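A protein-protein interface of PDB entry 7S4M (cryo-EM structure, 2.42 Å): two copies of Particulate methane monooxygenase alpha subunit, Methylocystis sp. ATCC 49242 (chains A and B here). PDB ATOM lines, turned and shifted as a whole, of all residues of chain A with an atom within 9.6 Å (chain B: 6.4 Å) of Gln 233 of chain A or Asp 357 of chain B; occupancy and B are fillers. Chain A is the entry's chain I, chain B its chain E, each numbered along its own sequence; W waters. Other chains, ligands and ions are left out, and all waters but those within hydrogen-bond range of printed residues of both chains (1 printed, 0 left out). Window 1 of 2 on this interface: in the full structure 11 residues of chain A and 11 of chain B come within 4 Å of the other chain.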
ATOM      1  N   PHE A  56      -6.205 -26.146 -18.714  1.00  0.00           N
ATOM      2  CA  PHE A  56      -7.129 -25.209 -18.096  1.00  0.00           C
ATOM      3  C   PHE A  56      -8.021 -25.940 -17.107  1.00  0.00           C
ATOM      4  O   PHE A  56      -8.583 -26.987 -17.435  1.00  0.00           O
ATOM      5  CB  PHE A  56      -7.986 -24.512 -19.151  1.00  0.00           C
ATOM      6  CG  PHE A  56      -8.842 -23.413 -18.605  1.00  0.00           C
ATOM      7  CD1 PHE A  56      -8.270 -22.261 -18.102  1.00  0.00           C
ATOM      8  CD2 PHE A  56     -10.217 -23.533 -18.588  1.00  0.00           C
ATOM      9  CE1 PHE A  56      -9.054 -21.249 -17.599  1.00  0.00           C
ATOM     10  CE2 PHE A  56     -11.005 -22.524 -18.087  1.00  0.00           C
ATOM     11  CZ  PHE A  56     -10.422 -21.380 -17.592  1.00  0.00           C
ATOM     12  N   PRO A  79      -7.378 -18.106 -13.584  1.00  0.00           N
ATOM     13  CA  PRO A  79      -8.400 -17.814 -14.592  1.00  0.00           C
ATOM     14  C   PRO A  79      -7.941 -18.093 -16.009  1.00  0.00           C
ATOM     15  O   PRO A  79      -8.773 -18.092 -16.924  1.00  0.00           O
ATOM     16  CB  PRO A  79      -8.660 -16.322 -14.388  1.00  0.00           C
ATOM     17  CG  PRO A  79      -7.349 -15.799 -13.953  1.00  0.00           C
ATOM     18  CD  PRO A  79      -6.707 -16.880 -13.122  1.00  0.00           C
ATOM     19  N   ARG A  80      -6.648 -18.330 -16.216  1.00  0.00           N
ATOM     20  CA  ARG A  80      -6.083 -18.585 -17.530  1.00  0.00           C
ATOM     21  C   ARG A  80      -5.456 -19.971 -17.543  1.00  0.00           C
ATOM     22  O   ARG A  80      -5.517 -20.714 -16.560  1.00  0.00           O
ATOM     23  CB  ARG A  80      -5.057 -17.509 -17.901  1.00  0.00           C
ATOM     24  CG  ARG A  80      -5.469 -16.111 -17.486  1.00  0.00           C
ATOM     25  CD  ARG A  80      -4.857 -15.066 -18.390  1.00  0.00           C
ATOM     26  NE  ARG A  80      -3.408 -15.008 -18.251  1.00  0.00           N
ATOM     27  CZ  ARG A  80      -2.760 -14.073 -17.571  1.00  0.00           C
ATOM     28  NH1 ARG A  80      -3.403 -13.094 -16.960  1.00  0.00           N
ATOM     29  NH2 ARG A  80      -1.434 -14.123 -17.506  1.00  0.00           N
ATOM     30  N   SER A  81      -4.848 -20.320 -18.672  1.00  0.00           N
ATOM     31  CA  SER A  81      -4.264 -21.643 -18.827  1.00  0.00           C
ATOM     32  C   SER A  81      -3.071 -21.821 -17.898  1.00  0.00           C
ATOM     33  O   SER A  81      -2.335 -20.877 -17.603  1.00  0.00           O
ATOM     34  CB  SER A  81      -3.840 -21.869 -20.273  1.00  0.00           C
ATOM     35  OG  SER A  81      -2.869 -20.918 -20.667  1.00  0.00           O
ATOM     36  N   THR A 229      -9.196   2.089 -20.335  1.00  0.00           N
ATOM     37  CA  THR A 229      -9.486   0.689 -20.583  1.00  0.00           C
ATOM     38  C   THR A 229      -8.184  -0.060 -20.822  1.00  0.00           C
ATOM     39  O   THR A 229      -7.148   0.534 -21.128  1.00  0.00           O
ATOM     40  CB  THR A 229     -10.414   0.516 -21.789  1.00  0.00           C
ATOM     41  OG1 THR A 229      -9.819   1.124 -22.940  1.00  0.00           O
ATOM     42  CG2 THR A 229     -11.759   1.165 -21.520  1.00  0.00           C
ATOM     43  N   ILE A 230      -8.243  -1.377 -20.674  1.00  0.00           N
ATOM     44  CA  ILE A 230      -7.055  -2.209 -20.832  1.00  0.00           C
ATOM     45  C   ILE A 230      -7.352  -3.324 -21.825  1.00  0.00           C
ATOM     46  O   ILE A 230      -8.513  -3.726 -21.977  1.00  0.00           O
ATOM     47  CB  ILE A 230      -6.595  -2.779 -19.484  1.00  0.00           C
ATOM     48  CG1 ILE A 230      -7.764  -3.436 -18.762  1.00  0.00           C
ATOM     49  CG2 ILE A 230      -5.996  -1.683 -18.626  1.00  0.00           C
ATOM     50  CD1 ILE A 230      -7.344  -4.529 -17.823  1.00  0.00           C
ATOM     51  N   PRO A 231      -6.349  -3.844 -22.525  1.00  0.00           N
ATOM     52  CA  PRO A 231      -6.588  -4.965 -23.435  1.00  0.00           C
ATOM     53  C   PRO A 231      -6.886  -6.243 -22.672  1.00  0.00           C
ATOM     54  O   PRO A 231      -6.632  -6.358 -21.471  1.00  0.00           O
ATOM     55  CB  PRO A 231      -5.275  -5.079 -24.211  1.00  0.00           C
ATOM     56  CG  PRO A 231      -4.261  -4.481 -23.309  1.00  0.00           C
ATOM     57  CD  PRO A 231      -4.957  -3.373 -22.587  1.00  0.00           C
ATOM     58  N   LEU A 232      -7.442  -7.212 -23.396  1.00  0.00           N
ATOM     59  CA  LEU A 232      -7.744  -8.508 -22.807  1.00  0.00           C
ATOM     60  C   LEU A 232      -6.486  -9.138 -22.228  1.00  0.00           C
ATOM     61  O   LEU A 232      -5.437  -9.171 -22.877  1.00  0.00           O
ATOM     62  CB  LEU A 232      -8.354  -9.434 -23.856  1.00  0.00           C
ATOM     63  CG  LEU A 232      -9.767  -9.103 -24.321  1.00  0.00           C
ATOM     64  CD1 LEU A 232     -10.116  -9.928 -25.538  1.00  0.00           C
ATOM     65  CD2 LEU A 232     -10.755  -9.353 -23.207  1.00  0.00           C
ATOM     66  N   GLN A 233      -6.596  -9.643 -21.005  1.00  0.00           N
ATOM     67  CA  GLN A 233      -5.467 -10.248 -20.309  1.00  0.00           C
ATOM     68  C   GLN A 233      -5.432 -11.732 -20.648  1.00  0.00           C
ATOM     69  O   GLN A 233      -6.362 -12.473 -20.319  1.00  0.00           O
ATOM     70  CB  GLN A 233      -5.585 -10.023 -18.807  1.00  0.00           C
ATOM     71  CG  GLN A 233      -5.658  -8.560 -18.427  1.00  0.00           C
ATOM     72  CD  GLN A 233      -4.413  -7.804 -18.826  1.00  0.00           C
ATOM     73  OE1 GLN A 233      -3.314  -8.113 -18.371  1.00  0.00           O
ATOM     74  NE2 GLN A 233      -4.575  -6.812 -19.691  1.00  0.00           N
ATOM     75  N   ALA A 234      -4.361 -12.164 -21.306  1.00  0.00           N
ATOM     76  CA  ALA A 234      -4.243 -13.538 -21.765  1.00  0.00           C
ATOM     77  C   ALA A 234      -2.804 -14.004 -21.612  1.00  0.00           C
ATOM     78  O   ALA A 234      -1.881 -13.201 -21.465  1.00  0.00           O
ATOM     79  CB  ALA A 234      -4.692 -13.687 -23.221  1.00  0.00           C
ATOM     80  N   GLY A 235      -2.626 -15.320 -21.649  1.00  0.00           N
ATOM     81  CA  GLY A 235      -1.301 -15.897 -21.574  1.00  0.00           C
ATOM     82  C   GLY A 235      -1.190 -17.015 -20.561  1.00  0.00           C
ATOM     83  O   GLY A 235      -1.921 -17.042 -19.567  1.00  0.00           O
ATOM     84  N   LEU A 236      -0.282 -17.951 -20.815  1.00  0.00           N
ATOM     85  CA  LEU A 236      -0.042 -19.032 -19.872  1.00  0.00           C
ATOM     86  C   LEU A 236       0.523 -18.480 -18.570  1.00  0.00           C
ATOM     87  O   LEU A 236       1.311 -17.532 -18.560  1.00  0.00           O
ATOM     88  CB  LEU A 236       0.918 -20.055 -20.480  1.00  0.00           C
ATOM     89  CG  LEU A 236       1.206 -21.315 -19.671  1.00  0.00           C
ATOM     90  CD1 LEU A 236      -0.019 -22.200 -19.621  1.00  0.00           C
ATOM     91  CD2 LEU A 236       2.375 -22.065 -20.272  1.00  0.00           C
ATOM     92  N   GLN A 237       0.107 -19.080 -17.463  1.00  0.00           N
ATOM     93  CA  GLN A 237       0.513 -18.620 -16.146  1.00  0.00           C
ATOM     94  C   GLN A 237       1.863 -19.216 -15.755  1.00  0.00           C
ATOM     95  O   GLN A 237       2.412 -20.081 -16.436  1.00  0.00           O
ATOM     96  CB  GLN A 237      -0.548 -18.975 -15.110  1.00  0.00           C
ATOM     97  CG  GLN A 237      -1.911 -18.406 -15.429  1.00  0.00           C
ATOM     98  CD  GLN A 237      -2.864 -18.498 -14.263  1.00  0.00           C
ATOM     99  OE1 GLN A 237      -3.989 -18.011 -14.331  1.00  0.00           O
ATOM    100  NE2 GLN A 237      -2.417 -19.120 -13.181  1.00  0.00           N
ATOM    101  N   LYS A 238       2.392 -18.737 -14.634  1.00  0.00           N
ATOM    102  CA  LYS A 238       3.662 -19.229 -14.133  1.00  0.00           C
ATOM    103  C   LYS A 238       3.508 -20.670 -13.652  1.00  0.00           C
ATOM    104  O   LYS A 238       2.401 -21.116 -13.346  1.00  0.00           O
ATOM    105  CB  LYS A 238       4.164 -18.335 -13.005  1.00  0.00           C
ATOM    106  CG  LYS A 238       3.342 -18.405 -11.739  1.00  0.00           C
ATOM    107  CD  LYS A 238       3.865 -17.430 -10.705  1.00  0.00           C
ATOM    108  CE  LYS A 238       3.427 -17.829  -9.310  1.00  0.00           C
ATOM    109  NZ  LYS A 238       4.063 -16.973  -8.275  1.00  0.00           N
ATOM    110  N   GLN B   7       7.360  -4.518 -25.959  1.00  0.00           N
ATOM    111  CA  GLN B   7       6.411  -4.572 -24.857  1.00  0.00           C
ATOM    112  C   GLN B   7       7.135  -4.717 -23.526  1.00  0.00           C
ATOM    113  O   GLN B   7       8.140  -5.425 -23.417  1.00  0.00           O
ATOM    114  CB  GLN B   7       5.429  -5.724 -25.059  1.00  0.00           C
ATOM    115  CG  GLN B   7       4.323  -5.396 -26.042  1.00  0.00           C
ATOM    116  CD  GLN B   7       3.202  -6.407 -26.022  1.00  0.00           C
ATOM    117  OE1 GLN B   7       3.347  -7.519 -26.521  1.00  0.00           O
ATOM    118  NE2 GLN B   7       2.071  -6.024 -25.442  1.00  0.00           N
ATOM    119  N   PHE B   9       6.252  -5.997 -20.429  1.00  0.00           N
ATOM    120  CA  PHE B   9       6.239  -7.242 -19.669  1.00  0.00           C
ATOM    121  C   PHE B   9       7.076  -8.318 -20.344  1.00  0.00           C
ATOM    122  O   PHE B   9       7.631  -9.184 -19.663  1.00  0.00           O
ATOM    123  CB  PHE B   9       4.806  -7.721 -19.457  1.00  0.00           C
ATOM    124  CG  PHE B   9       4.268  -8.557 -20.574  1.00  0.00           C
ATOM    125  CD1 PHE B   9       3.827  -7.970 -21.745  1.00  0.00           C
ATOM    126  CD2 PHE B   9       4.182  -9.930 -20.446  1.00  0.00           C
ATOM    127  CE1 PHE B   9       3.324  -8.739 -22.772  1.00  0.00           C
ATOM    128  CE2 PHE B   9       3.680 -10.703 -21.468  1.00  0.00           C
ATOM    129  CZ  PHE B   9       3.248 -10.107 -22.633  1.00  0.00           C
ATOM    130  N   ARG B  13      10.406  -9.918 -18.411  1.00  0.00           N
ATOM    131  CA  ARG B  13      10.159 -11.301 -18.014  1.00  0.00           C
ATOM    132  C   ARG B  13      10.777 -12.312 -18.972  1.00  0.00           C
ATOM    133  O   ARG B  13      10.348 -13.467 -19.000  1.00  0.00           O
ATOM    134  CB  ARG B  13       8.660 -11.564 -17.875  1.00  0.00           C
ATOM    135  CG  ARG B  13       7.956 -10.631 -16.916  1.00  0.00           C
ATOM    136  CD  ARG B  13       6.491 -10.987 -16.787  1.00  0.00           C
ATOM    137  NE  ARG B  13       6.220 -11.694 -15.543  1.00  0.00           N
ATOM    138  CZ  ARG B  13       5.662 -12.894 -15.471  1.00  0.00           C
ATOM    139  NH1 ARG B  13       5.292 -13.548 -16.559  1.00  0.00           N
ATOM    140  NH2 ARG B  13       5.472 -13.452 -14.281  1.00  0.00           N
ATOM    141  N   LEU B 352       3.177  -0.679 -19.323  1.00  0.00           N
ATOM    142  CA  LEU B 352       2.706  -2.004 -18.949  1.00  0.00           C
ATOM    143  C   LEU B 352       1.188  -2.100 -18.983  1.00  0.00           C
ATOM    144  O   LEU B 352       0.653  -3.196 -19.177  1.00  0.00           O
ATOM    145  CB  LEU B 352       3.233  -2.352 -17.560  1.00  0.00           C
ATOM    146  CG  LEU B 352       2.942  -3.738 -17.001  1.00  0.00           C
ATOM    147  CD1 LEU B 352       3.386  -4.796 -17.980  1.00  0.00           C
ATOM    148  CD2 LEU B 352       3.656  -3.907 -15.679  1.00  0.00           C
ATOM    149  N   ALA B 353       0.487  -0.980 -18.804  1.00  0.00           N
ATOM    150  CA  ALA B 353      -0.969  -0.995 -18.896  1.00  0.00           C
ATOM    151  C   ALA B 353      -1.437  -1.343 -20.301  1.00  0.00           C
ATOM    152  O   ALA B 353      -2.494  -1.962 -20.465  1.00  0.00           O
ATOM    153  CB  ALA B 353      -1.538   0.355 -18.470  1.00  0.00           C
ATOM    154  N   TYR B 354      -0.674  -0.956 -21.320  1.00  0.00           N
ATOM    155  CA  TYR B 354      -1.035  -1.277 -22.692  1.00  0.00           C
ATOM    156  C   TYR B 354      -0.844  -2.751 -23.020  1.00  0.00           C
ATOM    157  O   TYR B 354      -1.442  -3.241 -23.982  1.00  0.00           O
ATOM    158  CB  TYR B 354      -0.217  -0.420 -23.657  1.00  0.00           C
ATOM    159  CG  TYR B 354      -0.537  -0.657 -25.111  1.00  0.00           C
ATOM    160  CD1 TYR B 354      -1.623  -0.039 -25.710  1.00  0.00           C
ATOM    161  CD2 TYR B 354       0.251  -1.497 -25.888  1.00  0.00           C
ATOM    162  CE1 TYR B 354      -1.920  -0.254 -27.040  1.00  0.00           C
ATOM    163  CE2 TYR B 354      -0.038  -1.718 -27.216  1.00  0.00           C
ATOM    164  CZ  TYR B 354      -1.125  -1.095 -27.787  1.00  0.00           C
ATOM    165  OH  TYR B 354      -1.417  -1.307 -29.114  1.00  0.00           O
ATOM    166  N   ASP B 355      -0.043  -3.468 -22.241  1.00  0.00           N
ATOM    167  CA  ASP B 355       0.245  -4.861 -22.536  1.00  0.00           C
ATOM    168  C   ASP B 355      -0.932  -5.753 -22.160  1.00  0.00           C
ATOM    169  O   ASP B 355      -1.802  -5.384 -21.369  1.00  0.00           O
ATOM    170  CB  ASP B 355       1.501  -5.317 -21.800  1.00  0.00           C
ATOM    171  CG  ASP B 355       2.752  -4.634 -22.306  1.00  0.00           C
ATOM    172  OD1 ASP B 355       2.668  -3.926 -23.331  1.00  0.00           O
ATOM    173  OD2 ASP B 355       3.820  -4.801 -21.682  1.00  0.00           O
ATOM    174  N   THR B 356      -0.940  -6.949 -22.736  1.00  0.00           N
ATOM    175  CA  THR B 356      -1.974  -7.939 -22.476  1.00  0.00           C
ATOM    176  C   THR B 356      -1.685  -8.781 -21.242  1.00  0.00           C
ATOM    177  O   THR B 356      -2.425  -9.731 -20.972  1.00  0.00           O
ATOM    178  CB  THR B 356      -2.146  -8.860 -23.685  1.00  0.00           C
ATOM    179  OG1 THR B 356      -0.861  -9.179 -24.229  1.00  0.00           O
ATOM    180  CG2 THR B 356      -2.983  -8.180 -24.749  1.00  0.00           C
ATOM    181  N   ASP B 357      -0.625  -8.468 -20.499  1.00  0.00           N
ATOM    182  CA  ASP B 357      -0.302  -9.202 -19.280  1.00  0.00           C
ATOM    183  C   ASP B 357       0.390  -8.227 -18.332  1.00  0.00           C
ATOM    184  O   ASP B 357       1.592  -7.981 -18.463  1.00  0.00           O
ATOM    185  CB  ASP B 357       0.573 -10.410 -19.580  1.00  0.00           C
ATOM    186  CG  ASP B 357       0.334 -11.553 -18.620  1.00  0.00           C
ATOM    187  OD1 ASP B 357      -0.281 -11.320 -17.559  1.00  0.00           O
ATOM    188  OD2 ASP B 357       0.760 -12.686 -18.925  1.00  0.00           O
ATOM    189  N   SER B 358      -0.370  -7.680 -17.387  1.00  0.00           N
ATOM    190  CA  SER B 358       0.166  -6.725 -16.420  1.00  0.00           C
ATOM    191  C   SER B 358       0.964  -7.497 -15.374  1.00  0.00           C
ATOM    192  O   SER B 358       0.499  -7.786 -14.270  1.00  0.00           O
ATOM    193  CB  SER B 358      -0.955  -5.913 -15.789  1.00  0.00           C
ATOM    194  OG  SER B 358      -0.483  -4.652 -15.353  1.00  0.00           O
ATOM    195  N   GLN B 359       2.196  -7.838 -15.739  1.00  0.00           N
ATOM    196  CA  GLN B 359       3.065  -8.616 -14.870  1.00  0.00           C
ATOM    197  C   GLN B 359       4.478  -8.074 -14.981  1.00  0.00           C
ATOM    198  O   GLN B 359       4.956  -7.798 -16.083  1.00  0.00           O
ATOM    199  CB  GLN B 359       3.037 -10.099 -15.245  1.00  0.00           C
ATOM    200  CG  GLN B 359       1.977 -10.896 -14.522  1.00  0.00           C
ATOM    201  CD  GLN B 359       2.007 -12.363 -14.880  1.00  0.00           C
ATOM    202  OE1 GLN B 359       1.992 -13.227 -14.005  1.00  0.00           O
ATOM    203  NE2 GLN B 359       2.043 -12.655 -16.172  1.00  0.00           N
ATOM    204  N   ILE B 360       5.140  -7.923 -13.842  1.00  0.00           N
ATOM    205  CA  ILE B 360       6.498  -7.428 -13.804  1.00  0.00           C
ATOM    206  C   ILE B 360       7.460  -8.594 -13.615  1.00  0.00           C
ATOM    207  O   ILE B 360       7.065  -9.710 -13.292  1.00  0.00           O
ATOM    208  CB  ILE B 360       6.700  -6.367 -12.699  1.00  0.00           C
ATOM    209  CG1 ILE B 360       6.495  -6.989 -11.321  1.00  0.00           C
ATOM    210  CG2 ILE B 360       5.783  -5.188 -12.920  1.00  0.00           C
ATOM    211  CD1 ILE B 360       6.930  -6.098 -10.188  1.00  0.00           C
HETATM  212  O   HOH W   1      -2.776 -10.168 -15.652  1.00  0.00           O
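No position is printed for both chains. Of the 13 pairs that touch across the chains among the printed residues, none has its exchanged pair printed and touching as well.
Of the printed residues of chain B, Arg 80 of chain A touches Asp 357 (3.0 Å). Ser 81 of chain A touches none of the printed residues of chain B. Thr 229 of chain A touches none of the printed residues of chain B. Printed residues of chain B within 4 Å of Pro 231 of chain A: Ala 353 (3.5 Å), Tyr 354 (3.2 Å), Asp 355 (3.3 Å) and Thr 356 (3.9 Å). Of the printed residues of chain B, Gln 233 of chain A touches Asp 355, Thr 356, Asp 357 and Ser 358. Of the printed residues of chain A, Tyr 354 of chain B touches Pro 231. Of the printed residues of chain A, Asp 355 of chain B touches Pro 231 and Gln 233. Of chain A, only Arg 80, Gln 233 and Ala 234 come within 4 Å of Asp 357 of chain B.
Water W1 lies within hydrogen-bond range of NH1 of Arg 80 of chain A (3.3 Å), OD1 of Asp 357 of chain B (3.3 Å) and OE1 of Gln 233 of chain A (3.5 Å).
Of the 14 printed residues of chain A, 6 touch a printed residue of chain B. Printed residues of chain A that touch a printed residue of chain B: Arg 80, Ile 230, Pro 231, Leu 232, Gln 233 and Ala 234. Printed residues of chain B that touch a printed residue of chain A: Ala 353, Tyr 354, Asp 355, Thr 356, Asp 357 and Ser 358. Along chain B the printed residues that touch a printed residue of chain A span positions 353 to 358. Among the printed residues, 13 pairs touch across the chains.
CG2 of Ile 230 of chain A touches O of Ala 353 of chain B (3.97 Å). Pro 231 of chain A touches Ala 353 of chain B (CD to O, 3.5 Å). Pro 231 of chain A touches Tyr 354 of chain B (CG to O, 3.2 Å). O of Asp 355 of chain B touches CG of Pro 231 of chain A (3.3 Å). Pro 231 of chain A touches Thr 356 of chain B. Thr 356 of chain B touches Leu 232 of chain A (CG2 to O, 3.2 Å). Asp 355 of chain B touches Gln 233 of chain A. Asp 357 of chain B touches Ala 234 of chain A.
The side-chain amide oxygen (OE1) of Gln 233 of chain A sits close to the backbone carbonyl oxygen (O) of Thr 356 of chain B. O of Thr 356 of chain B is in hydrogen-bond range of N of Ala 234 of chain A (3.1 Å). NH2 of Arg 80 of chain A is in salt-bridge range of OD2 of Asp 357 of chain B (3.0 Å). The backbone NH (N) of Asp 357 of chain B lies close to the side-chain amide oxygen (OE1) of Gln 233 of chain A (3.4 Å). N of Ser 358 of chain B lies within hydrogen-bond range of OE1 of Gln 233 of chain A, at 3.1 Å.
The side-chain amide nitrogen (NE2) of Gln 7 of chain B is in hydrogen-bond range of the side-chain carboxylate (OD1) of Asp 355 of chain B, at 3.0 Å. The backbone NH (N) of Phe 9 of chain B sits at hydrogen-bond distance from the side-chain carboxylate (OD2) of Asp 355 of chain B (3.0 Å). The side-chain carboxylate (OD1) of Asp 357 of chain B lies within hydrogen-bond range of the side-chain amide nitrogen (NE2) of Gln 359 of chain B (3.0 Å). NE of Arg 80 of chain A is in hydrogen-bond range of O of Gly 235 of chain A (2.8 Å). The backbone NH (N) of Arg 80 of chain A sits at hydrogen-bond distance from the side-chain amide oxygen (OE1) of Gln 237 of chain A (3.3 Å). O of Pro 231 of chain A sits at hydrogen-bond distance from NE2 of Gln 233 of chain A, 2.8 Å away.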
